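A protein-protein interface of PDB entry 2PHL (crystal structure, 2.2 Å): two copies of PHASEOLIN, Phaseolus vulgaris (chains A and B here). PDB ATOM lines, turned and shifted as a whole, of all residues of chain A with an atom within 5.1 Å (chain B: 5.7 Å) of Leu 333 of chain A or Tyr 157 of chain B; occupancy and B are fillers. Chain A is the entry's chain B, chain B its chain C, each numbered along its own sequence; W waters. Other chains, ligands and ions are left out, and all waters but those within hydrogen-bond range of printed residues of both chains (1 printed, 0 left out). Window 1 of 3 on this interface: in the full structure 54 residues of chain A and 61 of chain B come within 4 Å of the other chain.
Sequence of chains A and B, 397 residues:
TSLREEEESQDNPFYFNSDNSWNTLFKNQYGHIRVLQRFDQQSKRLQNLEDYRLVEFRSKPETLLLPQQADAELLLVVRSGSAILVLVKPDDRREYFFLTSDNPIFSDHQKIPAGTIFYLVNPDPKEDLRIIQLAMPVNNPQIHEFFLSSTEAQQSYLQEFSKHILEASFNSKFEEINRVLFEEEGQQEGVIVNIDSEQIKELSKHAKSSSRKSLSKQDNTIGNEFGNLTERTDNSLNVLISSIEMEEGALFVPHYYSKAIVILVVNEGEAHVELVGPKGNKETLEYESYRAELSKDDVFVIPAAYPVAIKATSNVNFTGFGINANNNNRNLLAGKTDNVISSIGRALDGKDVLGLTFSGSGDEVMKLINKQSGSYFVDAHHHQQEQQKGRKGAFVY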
ATOM      1  N   VAL A 253      23.775   2.582  30.488  1.00  0.00           N
ATOM      2  CA  VAL A 253      23.072   3.843  30.706  1.00  0.00           C
ATOM      3  C   VAL A 253      21.650   3.818  30.163  1.00  0.00           C
ATOM      4  O   VAL A 253      21.340   3.034  29.247  1.00  0.00           O
ATOM      5  CB  VAL A 253      23.840   5.049  30.028  1.00  0.00           C
ATOM      6  CG1 VAL A 253      25.288   5.154  30.531  1.00  0.00           C
ATOM      7  CG2 VAL A 253      23.791   4.940  28.498  1.00  0.00           C
ATOM      8  N   PRO A 254      20.765   4.671  30.725  1.00  0.00           N
ATOM      9  CA  PRO A 254      19.365   4.768  30.295  1.00  0.00           C
ATOM     10  C   PRO A 254      19.293   4.890  28.772  1.00  0.00           C
ATOM     11  O   PRO A 254      20.149   5.524  28.132  1.00  0.00           O
ATOM     12  CB  PRO A 254      18.895   6.048  30.977  1.00  0.00           C
ATOM     13  CG  PRO A 254      19.607   6.005  32.259  1.00  0.00           C
ATOM     14  CD  PRO A 254      21.014   5.572  31.868  1.00  0.00           C
ATOM     15  N   HIS A 255      18.287   4.246  28.199  1.00  0.00           N
ATOM     16  CA  HIS A 255      18.081   4.221  26.764  1.00  0.00           C
ATOM     17  C   HIS A 255      16.748   3.541  26.492  1.00  0.00           C
ATOM     18  O   HIS A 255      16.097   3.104  27.421  1.00  0.00           O
ATOM     19  CB  HIS A 255      19.197   3.396  26.125  1.00  0.00           C
ATOM     20  CG  HIS A 255      19.197   1.951  26.534  1.00  0.00           C
ATOM     21  ND1 HIS A 255      19.697   1.523  27.744  1.00  0.00           N
ATOM     22  CD2 HIS A 255      18.764   0.844  25.891  1.00  0.00           C
ATOM     23  CE1 HIS A 255      19.574   0.212  27.829  1.00  0.00           C
ATOM     24  NE2 HIS A 255      19.007  -0.226  26.715  1.00  0.00           N
ATOM     25  N   TYR A 256      16.323   3.508  25.232  1.00  0.00           N
ATOM     26  CA  TYR A 256      15.092   2.820  24.833  1.00  0.00           C
ATOM     27  C   TYR A 256      15.216   2.432  23.360  1.00  0.00           C
ATOM     28  O   TYR A 256      16.005   3.022  22.614  1.00  0.00           O
ATOM     29  CB  TYR A 256      13.834   3.680  25.060  1.00  0.00           C
ATOM     30  CG  TYR A 256      13.634   4.840  24.091  1.00  0.00           C
ATOM     31  CD1 TYR A 256      13.154   4.632  22.797  1.00  0.00           C
ATOM     32  CD2 TYR A 256      13.935   6.157  24.466  1.00  0.00           C
ATOM     33  CE1 TYR A 256      12.981   5.704  21.895  1.00  0.00           C
ATOM     34  CE2 TYR A 256      13.772   7.240  23.559  1.00  0.00           C
ATOM     35  CZ  TYR A 256      13.299   7.001  22.282  1.00  0.00           C
ATOM     36  OH  TYR A 256      13.184   8.048  21.378  1.00  0.00           O
ATOM     37  N   VAL A 276      11.214   2.298  33.367  1.00  0.00           N
ATOM     38  CA  VAL A 276      10.244   3.358  33.586  1.00  0.00           C
ATOM     39  C   VAL A 276       9.082   3.093  32.630  1.00  0.00           C
ATOM     40  O   VAL A 276       9.242   3.120  31.418  1.00  0.00           O
ATOM     41  CB  VAL A 276      10.858   4.763  33.309  1.00  0.00           C
ATOM     42  CG1 VAL A 276       9.903   5.854  33.737  1.00  0.00           C
ATOM     43  CG2 VAL A 276      12.163   4.928  34.055  1.00  0.00           C
ATOM     44  N   TYR A 287       4.431   8.408  35.676  1.00  0.00           N
ATOM     45  CA  TYR A 287       5.268   7.232  35.535  1.00  0.00           C
ATOM     46  C   TYR A 287       5.395   6.420  36.801  1.00  0.00           C
ATOM     47  O   TYR A 287       4.671   6.628  37.773  1.00  0.00           O
ATOM     48  CB  TYR A 287       6.639   7.595  34.969  1.00  0.00           C
ATOM     49  CG  TYR A 287       6.522   8.339  33.669  1.00  0.00           C
ATOM     50  CD1 TYR A 287       5.926   7.747  32.552  1.00  0.00           C
ATOM     51  CD2 TYR A 287       6.877   9.686  33.594  1.00  0.00           C
ATOM     52  CE1 TYR A 287       5.667   8.488  31.406  1.00  0.00           C
ATOM     53  CE2 TYR A 287       6.627  10.440  32.449  1.00  0.00           C
ATOM     54  CZ  TYR A 287       6.016   9.841  31.369  1.00  0.00           C
ATOM     55  OH  TYR A 287       5.698  10.632  30.290  1.00  0.00           O
ATOM     56  N   PRO A 307      12.026   3.392  28.623  1.00  0.00           N
ATOM     57  CA  PRO A 307      13.431   3.572  29.036  1.00  0.00           C
ATOM     58  C   PRO A 307      13.908   2.539  30.058  1.00  0.00           C
ATOM     59  O   PRO A 307      13.213   2.212  31.017  1.00  0.00           O
ATOM     60  CB  PRO A 307      13.435   4.991  29.634  1.00  0.00           C
ATOM     61  CG  PRO A 307      12.227   5.660  28.989  1.00  0.00           C
ATOM     62  CD  PRO A 307      11.209   4.535  29.050  1.00  0.00           C
ATOM     63  N   ASN A 331      18.077   4.574  21.113  1.00  0.00           N
ATOM     64  CA  ASN A 331      18.164   5.959  21.592  1.00  0.00           C
ATOM     65  C   ASN A 331      18.729   6.011  22.994  1.00  0.00           C
ATOM     66  O   ASN A 331      18.070   5.571  23.943  1.00  0.00           O
ATOM     67  CB  ASN A 331      16.792   6.643  21.601  1.00  0.00           C
ATOM     68  CG  ASN A 331      16.233   6.853  20.209  1.00  0.00           C
ATOM     69  OD1 ASN A 331      16.523   7.852  19.554  1.00  0.00           O
ATOM     70  ND2 ASN A 331      15.427   5.909  19.745  1.00  0.00           N
ATOM     71  N   LEU A 332      19.934   6.581  23.120  1.00  0.00           N
ATOM     72  CA  LEU A 332      20.631   6.719  24.396  1.00  0.00           C
ATOM     73  C   LEU A 332      20.427   8.066  25.080  1.00  0.00           C
ATOM     74  O   LEU A 332      20.363   9.116  24.427  1.00  0.00           O
ATOM     75  CB  LEU A 332      22.111   6.428  24.213  1.00  0.00           C
ATOM     76  CG  LEU A 332      22.432   4.931  24.127  1.00  0.00           C
ATOM     77  CD1 LEU A 332      21.848   4.255  22.879  1.00  0.00           C
ATOM     78  CD2 LEU A 332      23.918   4.751  24.195  1.00  0.00           C
ATOM     79  N   LEU A 333      20.370   8.032  26.407  1.00  0.00           N
ATOM     80  CA  LEU A 333      20.129   9.228  27.186  1.00  0.00           C
ATOM     81  C   LEU A 333      21.305   9.728  28.017  1.00  0.00           C
ATOM     82  O   LEU A 333      21.124  10.503  28.963  1.00  0.00           O
ATOM     83  CB  LEU A 333      18.902   9.006  28.070  1.00  0.00           C
ATOM     84  CG  LEU A 333      17.583   8.759  27.326  1.00  0.00           C
ATOM     85  CD1 LEU A 333      16.669   7.856  28.152  1.00  0.00           C
ATOM     86  CD2 LEU A 333      16.901  10.096  26.991  1.00  0.00           C
ATOM     87  N   ALA A 334      22.505   9.284  27.658  1.00  0.00           N
ATOM     88  CA  ALA A 334      23.733   9.686  28.338  1.00  0.00           C
ATOM     89  C   ALA A 334      24.853   9.187  27.449  1.00  0.00           C
ATOM     90  O   ALA A 334      24.611   8.341  26.590  1.00  0.00           O
ATOM     91  CB  ALA A 334      23.819   9.046  29.723  1.00  0.00           C
ATOM     92  N   GLY A 335      26.064   9.714  27.625  1.00  0.00           N
ATOM     93  CA  GLY A 335      27.180   9.275  26.795  1.00  0.00           C
ATOM     94  C   GLY A 335      27.377  10.075  25.510  1.00  0.00           C
ATOM     95  O   GLY A 335      26.523  10.910  25.123  1.00  0.00           O
ATOM     96  N   ASN A 339      23.237   9.739  21.572  1.00  0.00           N
ATOM     97  CA  ASN A 339      22.532  10.525  22.578  1.00  0.00           C
ATOM     98  C   ASN A 339      21.516  11.477  21.946  1.00  0.00           C
ATOM     99  O   ASN A 339      21.880  12.481  21.341  1.00  0.00           O
ATOM    100  CB  ASN A 339      23.540  11.298  23.446  1.00  0.00           C
ATOM    101  CG  ASN A 339      22.881  12.037  24.596  1.00  0.00           C
ATOM    102  OD1 ASN A 339      21.804  12.612  24.435  1.00  0.00           O
ATOM    103  ND2 ASN A 339      23.537  12.055  25.755  1.00  0.00           N
ATOM    104  N   VAL A 340      20.236  11.169  22.134  1.00  0.00           N
ATOM    105  CA  VAL A 340      19.159  11.986  21.583  1.00  0.00           C
ATOM    106  C   VAL A 340      19.015  13.372  22.167  1.00  0.00           C
ATOM    107  O   VAL A 340      18.515  14.256  21.489  1.00  0.00           O
ATOM    108  CB  VAL A 340      17.782  11.324  21.708  1.00  0.00           C
ATOM    109  CG1 VAL A 340      17.535  10.457  20.526  1.00  0.00           C
ATOM    110  CG2 VAL A 340      17.673  10.553  23.017  1.00  0.00           C
ATOM    111  N   ILE A 341      19.386  13.550  23.434  1.00  0.00           N
ATOM    112  CA  ILE A 341      19.280  14.854  24.085  1.00  0.00           C
ATOM    113  C   ILE A 341      20.265  15.835  23.470  1.00  0.00           C
ATOM    114  O   ILE A 341      19.938  17.009  23.297  1.00  0.00           O
ATOM    115  CB  ILE A 341      19.484  14.767  25.595  1.00  0.00           C
ATOM    116  CG1 ILE A 341      18.482  13.780  26.197  1.00  0.00           C
ATOM    117  CG2 ILE A 341      19.230  16.115  26.216  1.00  0.00           C
ATOM    118  CD1 ILE A 341      18.498  13.741  27.700  1.00  0.00           C
ATOM    119  N   ILE A 369      25.422  17.413  29.765  1.00  0.00           N
ATOM    120  CA  ILE A 369      25.326  16.318  28.808  1.00  0.00           C
ATOM    121  C   ILE A 369      26.682  15.921  28.232  1.00  0.00           C
ATOM    122  O   ILE A 369      26.864  14.793  27.786  1.00  0.00           O
ATOM    123  CB  ILE A 369      24.264  16.631  27.708  1.00  0.00           C
ATOM    124  CG1 ILE A 369      23.472  15.384  27.379  1.00  0.00           C
ATOM    125  CG2 ILE A 369      24.902  17.172  26.448  1.00  0.00           C
ATOM    126  CD1 ILE A 369      22.662  14.874  28.529  1.00  0.00           C
ATOM    127  N   GLN B  69       8.433  10.935  22.987  1.00  0.00           N
ATOM    128  CA  GLN B  69       8.415   9.792  22.105  1.00  0.00           C
ATOM    129  C   GLN B  69       7.180   9.000  22.574  1.00  0.00           C
ATOM    130  O   GLN B  69       6.808   9.064  23.754  1.00  0.00           O
ATOM    131  CB  GLN B  69       9.711   8.983  22.230  1.00  0.00           C
ATOM    132  CG  GLN B  69       9.690   7.887  23.263  1.00  0.00           C
ATOM    133  CD  GLN B  69      10.347   8.266  24.555  1.00  0.00           C
ATOM    134  OE1 GLN B  69      10.355   7.485  25.497  1.00  0.00           O
ATOM    135  NE2 GLN B  69      10.922   9.451  24.610  1.00  0.00           N
ATOM    136  N   ILE B 117      11.512  10.715  18.844  1.00  0.00           N
ATOM    137  CA  ILE B 117      11.378  11.930  19.658  1.00  0.00           C
ATOM    138  C   ILE B 117      10.908  13.015  18.730  1.00  0.00           C
ATOM    139  O   ILE B 117      11.438  13.131  17.636  1.00  0.00           O
ATOM    140  CB  ILE B 117      12.746  12.405  20.236  1.00  0.00           C
ATOM    141  CG1 ILE B 117      13.181  11.534  21.425  1.00  0.00           C
ATOM    142  CG2 ILE B 117      12.651  13.897  20.650  1.00  0.00           C
ATOM    143  CD1 ILE B 117      12.453  11.885  22.752  1.00  0.00           C
ATOM    144  N   PHE B 146       5.807   9.360  26.381  1.00  0.00           N
ATOM    145  CA  PHE B 146       6.811   9.684  27.376  1.00  0.00           C
ATOM    146  C   PHE B 146       7.354  11.084  27.155  1.00  0.00           C
ATOM    147  O   PHE B 146       7.974  11.350  26.136  1.00  0.00           O
ATOM    148  CB  PHE B 146       7.946   8.682  27.315  1.00  0.00           C
ATOM    149  CG  PHE B 146       7.523   7.288  27.648  1.00  0.00           C
ATOM    150  CD1 PHE B 146       6.804   6.531  26.728  1.00  0.00           C
ATOM    151  CD2 PHE B 146       7.804   6.740  28.903  1.00  0.00           C
ATOM    152  CE1 PHE B 146       6.362   5.249  27.042  1.00  0.00           C
ATOM    153  CE2 PHE B 146       7.368   5.458  29.230  1.00  0.00           C
ATOM    154  CZ  PHE B 146       6.643   4.714  28.288  1.00  0.00           C
ATOM    155  N   PHE B 147       7.091  11.984  28.097  1.00  0.00           N
ATOM    156  CA  PHE B 147       7.573  13.359  28.028  1.00  0.00           C
ATOM    157  C   PHE B 147       8.943  13.531  28.703  1.00  0.00           C
ATOM    158  O   PHE B 147       9.166  13.074  29.834  1.00  0.00           O
ATOM    159  CB  PHE B 147       6.535  14.314  28.623  1.00  0.00           C
ATOM    160  CG  PHE B 147       5.518  14.807  27.620  1.00  0.00           C
ATOM    161  CD1 PHE B 147       5.813  15.877  26.781  1.00  0.00           C
ATOM    162  CD2 PHE B 147       4.266  14.204  27.513  1.00  0.00           C
ATOM    163  CE1 PHE B 147       4.874  16.346  25.842  1.00  0.00           C
ATOM    164  CE2 PHE B 147       3.323  14.665  26.585  1.00  0.00           C
ATOM    165  CZ  PHE B 147       3.631  15.742  25.746  1.00  0.00           C
ATOM    166  N   LEU B 148       9.876  14.131  27.968  1.00  0.00           N
ATOM    167  CA  LEU B 148      11.248  14.363  28.436  1.00  0.00           C
ATOM    168  C   LEU B 148      11.328  15.505  29.423  1.00  0.00           C
ATOM    169  O   LEU B 148      12.270  15.602  30.200  1.00  0.00           O
ATOM    170  CB  LEU B 148      12.153  14.716  27.254  1.00  0.00           C
ATOM    171  CG  LEU B 148      13.525  14.053  27.123  1.00  0.00           C
ATOM    172  CD1 LEU B 148      14.442  14.993  26.405  1.00  0.00           C
ATOM    173  CD2 LEU B 148      14.108  13.688  28.457  1.00  0.00           C
ATOM    174  N   SER B 149      10.353  16.398  29.341  1.00  0.00           N
ATOM    175  CA  SER B 149      10.280  17.584  30.183  1.00  0.00           C
ATOM    176  C   SER B 149       9.994  17.409  31.684  1.00  0.00           C
ATOM    177  O   SER B 149       9.457  16.383  32.140  1.00  0.00           O
ATOM    178  CB  SER B 149       9.242  18.544  29.589  1.00  0.00           C
ATOM    179  OG  SER B 149       8.134  17.835  29.063  1.00  0.00           O
ATOM    180  N   GLN B 155       6.554  15.064  35.659  1.00  0.00           N
ATOM    181  CA  GLN B 155       7.978  14.891  35.831  1.00  0.00           C
ATOM    182  C   GLN B 155       8.529  14.155  34.624  1.00  0.00           C
ATOM    183  O   GLN B 155       7.795  13.497  33.873  1.00  0.00           O
ATOM    184  CB  GLN B 155       8.302  14.149  37.131  1.00  0.00           C
ATOM    185  CG  GLN B 155       7.923  14.949  38.383  1.00  0.00           C
ATOM    186  CD  GLN B 155       8.273  14.249  39.685  1.00  0.00           C
ATOM    187  OE1 GLN B 155       8.588  14.897  40.681  1.00  0.00           O
ATOM    188  NE2 GLN B 155       8.200  12.923  39.692  1.00  0.00           N
ATOM    189  N   SER B 156       9.817  14.339  34.398  1.00  0.00           N
ATOM    190  CA  SER B 156      10.477  13.694  33.296  1.00  0.00           C
ATOM    191  C   SER B 156      10.738  12.227  33.672  1.00  0.00           C
ATOM    192  O   SER B 156      10.953  11.923  34.859  1.00  0.00           O
ATOM    193  CB  SER B 156      11.786  14.417  33.029  1.00  0.00           C
ATOM    194  OG  SER B 156      12.475  13.748  32.012  1.00  0.00           O
ATOM    195  N   TYR B 157      10.702  11.318  32.690  1.00  0.00           N
ATOM    196  CA  TYR B 157      10.981   9.908  32.972  1.00  0.00           C
ATOM    197  C   TYR B 157      12.417   9.739  33.441  1.00  0.00           C
ATOM    198  O   TYR B 157      12.789   8.699  33.977  1.00  0.00           O
ATOM    199  CB  TYR B 157      10.659   8.982  31.785  1.00  0.00           C
ATOM    200  CG  TYR B 157      11.232   9.370  30.445  1.00  0.00           C
ATOM    201  CD1 TYR B 157      12.543   9.045  30.097  1.00  0.00           C
ATOM    202  CD2 TYR B 157      10.441  10.018  29.502  1.00  0.00           C
ATOM    203  CE1 TYR B 157      13.042   9.355  28.842  1.00  0.00           C
ATOM    204  CE2 TYR B 157      10.926  10.335  28.238  1.00  0.00           C
ATOM    205  CZ  TYR B 157      12.220  10.000  27.907  1.00  0.00           C
ATOM    206  OH  TYR B 157      12.660  10.246  26.621  1.00  0.00           O
ATOM    207  N   LEU B 158      13.213  10.793  33.278  1.00  0.00           N
ATOM    208  CA  LEU B 158      14.589  10.773  33.740  1.00  0.00           C
ATOM    209  C   LEU B 158      14.527  10.662  35.258  1.00  0.00           C
ATOM    210  O   LEU B 158      15.134   9.769  35.838  1.00  0.00           O
ATOM    211  CB  LEU B 158      15.320  12.043  33.296  1.00  0.00           C
ATOM    212  CG  LEU B 158      15.677  12.060  31.797  1.00  0.00           C
ATOM    213  CD1 LEU B 158      16.289  13.375  31.389  1.00  0.00           C
ATOM    214  CD2 LEU B 158      16.632  10.913  31.483  1.00  0.00           C
ATOM    215  N   GLN B 159      13.667  11.484  35.867  1.00  0.00           N
ATOM    216  CA  GLN B 159      13.444  11.526  37.333  1.00  0.00           C
ATOM    217  C   GLN B 159      13.029  10.180  37.980  1.00  0.00           C
ATOM    218  O   GLN B 159      12.948  10.065  39.197  1.00  0.00           O
ATOM    219  CB  GLN B 159      12.360  12.581  37.670  1.00  0.00           C
ATOM    220  CG  GLN B 159      12.870  13.948  38.119  1.00  0.00           C
ATOM    221  CD  GLN B 159      11.808  15.070  38.002  1.00  0.00           C
ATOM    222  OE1 GLN B 159      11.236  15.515  39.002  1.00  0.00           O
ATOM    223  NE2 GLN B 159      11.564  15.535  36.776  1.00  0.00           N
ATOM    224  N   GLU B 160      12.772   9.170  37.167  1.00  0.00           N
ATOM    225  CA  GLU B 160      12.335   7.896  37.682  1.00  0.00           C
ATOM    226  C   GLU B 160      13.414   6.852  37.947  1.00  0.00           C
ATOM    227  O   GLU B 160      13.110   5.767  38.456  1.00  0.00           O
ATOM    228  CB  GLU B 160      11.264   7.340  36.758  1.00  0.00           C
ATOM    229  CG  GLU B 160       9.983   8.141  36.778  1.00  0.00           C
ATOM    230  CD  GLU B 160       9.221   7.985  38.071  1.00  0.00           C
ATOM    231  OE1 GLU B 160       9.527   7.057  38.857  1.00  0.00           O
ATOM    232  OE2 GLU B 160       8.307   8.804  38.300  1.00  0.00           O
ATOM    233  N   PHE B 161      14.653   7.141  37.547  1.00  0.00           N
ATOM    234  CA  PHE B 161      15.765   6.218  37.788  1.00  0.00           C
ATOM    235  C   PHE B 161      16.389   6.597  39.113  1.00  0.00           C
ATOM    236  O   PHE B 161      16.126   7.669  39.652  1.00  0.00           O
ATOM    237  CB  PHE B 161      16.821   6.295  36.691  1.00  0.00           C
ATOM    238  CG  PHE B 161      16.395   5.685  35.387  1.00  0.00           C
ATOM    239  CD1 PHE B 161      16.086   4.326  35.301  1.00  0.00           C
ATOM    240  CD2 PHE B 161      16.339   6.456  34.231  1.00  0.00           C
ATOM    241  CE1 PHE B 161      15.729   3.737  34.081  1.00  0.00           C
ATOM    242  CE2 PHE B 161      15.984   5.875  33.004  1.00  0.00           C
ATOM    243  CZ  PHE B 161      15.680   4.512  32.934  1.00  0.00           C
ATOM    244  N   PHE B 170      25.461  10.371  34.040  1.00  0.00           N
ATOM    245  CA  PHE B 170      25.879  11.723  33.683  1.00  0.00           C
ATOM    246  C   PHE B 170      27.264  12.140  34.179  1.00  0.00           C
ATOM    247  O   PHE B 170      27.753  13.216  33.795  1.00  0.00           O
ATOM    248  CB  PHE B 170      24.835  12.738  34.146  1.00  0.00           C
ATOM    249  CG  PHE B 170      23.553  12.661  33.388  1.00  0.00           C
ATOM    250  CD1 PHE B 170      23.502  13.026  32.048  1.00  0.00           C
ATOM    251  CD2 PHE B 170      22.398  12.194  33.994  1.00  0.00           C
ATOM    252  CE1 PHE B 170      22.317  12.921  31.322  1.00  0.00           C
ATOM    253  CE2 PHE B 170      21.210  12.087  33.275  1.00  0.00           C
ATOM    254  CZ  PHE B 170      21.171  12.452  31.932  1.00  0.00           C
HETATM  255  O   HOH W   1      14.231   9.552  18.539  1.00  0.00           O
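Tyr 256 of chain A touches Gln 69 of chain B (OH to CB, 3.7 Å).
Val 276 of chain A touches Phe 146 of chain B.
Phe 161 of chain B touches Val 276 of chain A.
Tyr 287 of chain A touches Phe 146 of chain B.
CE2 of Tyr 287 of chain A touches O of Gln 155 of chain B (3.6 Å).
Tyr 287 of chain A touches Glu 160 of chain B.
Pro 307 of chain A touches Phe 146 of chain B (CD to CE2, 3.95 Å).
Pro 307 of chain A touches Phe 161 of chain B (O to CZ, 3.9 Å).
Phe 170 of chain B touches Leu 333 of chain A (CZ to O, 3.6 Å).
Ile 369 of chain A touches Phe 170 of chain B.
Of the 16 printed residues of chain A, 7 touch a printed residue of chain B.
Hydrophobic or aromatic side chains of chain A that line the printed part of chain B: Pro 254, Tyr 256, Val 276, Tyr 287, Pro 307, Leu 333 and Ile 369.
Of the 14 printed residues of chain B, 9 touch a printed residue of chain A.
Printed residues of chain B that touch a printed residue of chain A: Gln 69, Ile 117, Phe 146, Phe 147, Gln 155, Tyr 157, Glu 160, Phe 161 and Phe 170.
Hydrophobic or aromatic side chains of chain B that line the printed part of chain A: Ile 117, Phe 146, Tyr 157, Phe 161 and Phe 170.
No position is printed for both chains.
Of the 17 pairs that touch across the chains among the printed residues, none has its exchanged pair printed and touching as well.
Water W1 lies within hydrogen-bond range of N of Ile 117 of chain B (3.0 Å), OD1 of Asn 331 of chain A (3.0 Å) and OH of Tyr 256 of chain A (3.4 Å).
O of Pro 307 of chain A is in hydrogen-bond range of N of Val 276 of chain A.
O of Gln 69 of chain B sits at hydrogen-bond distance from N of Phe 146 of chain B.
The backbone carbonyl oxygen (O) of Tyr 256 of chain A lies within hydrogen-bond range of the backbone NH (N) of Asn 331 of chain A (3.0 Å).
The side-chain amide oxygen of Gln 159 of chain B sits close to the side-chain amide oxygen of Gln 155 of chain B, at 3.2 Å.
O of Pro 254 of chain A sits at hydrogen-bond distance from N of Leu 333 of chain A, at 3.1 Å.
OH of Tyr 157 of chain B lies within hydrogen-bond range of NE2 of Gln 69 of chain B (2.8 Å).
Printed residues of chain B within 4 Å of Leu 333 of chain A: Tyr 157 and Phe 170.
Of the printed residues of chain A, Ile 117 of chain B touches Tyr 256.
Of the printed residues of chain A, Gln 155 of chain B touches Tyr 287 (3.6 Å).
Of the printed residues of chain A, Glu 160 of chain B touches Val 276 and Tyr 287.
Printed residues of chain B within 4 Å of Ile 369 of chain A: Phe 170.
The nearest printed residue of chain B that does not touch Leu 333 of chain A is Leu 158 of chain B (4.5 Å).
The nearest printed residue of chain B that does not touch Ile 369 of chain A is Leu 158 of chain B (7.1 Å).
The side-chain hydroxyl of Tyr 287 of chain A lies within hydrogen-bond range of the backbone NH of Phe 147 of chain B.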
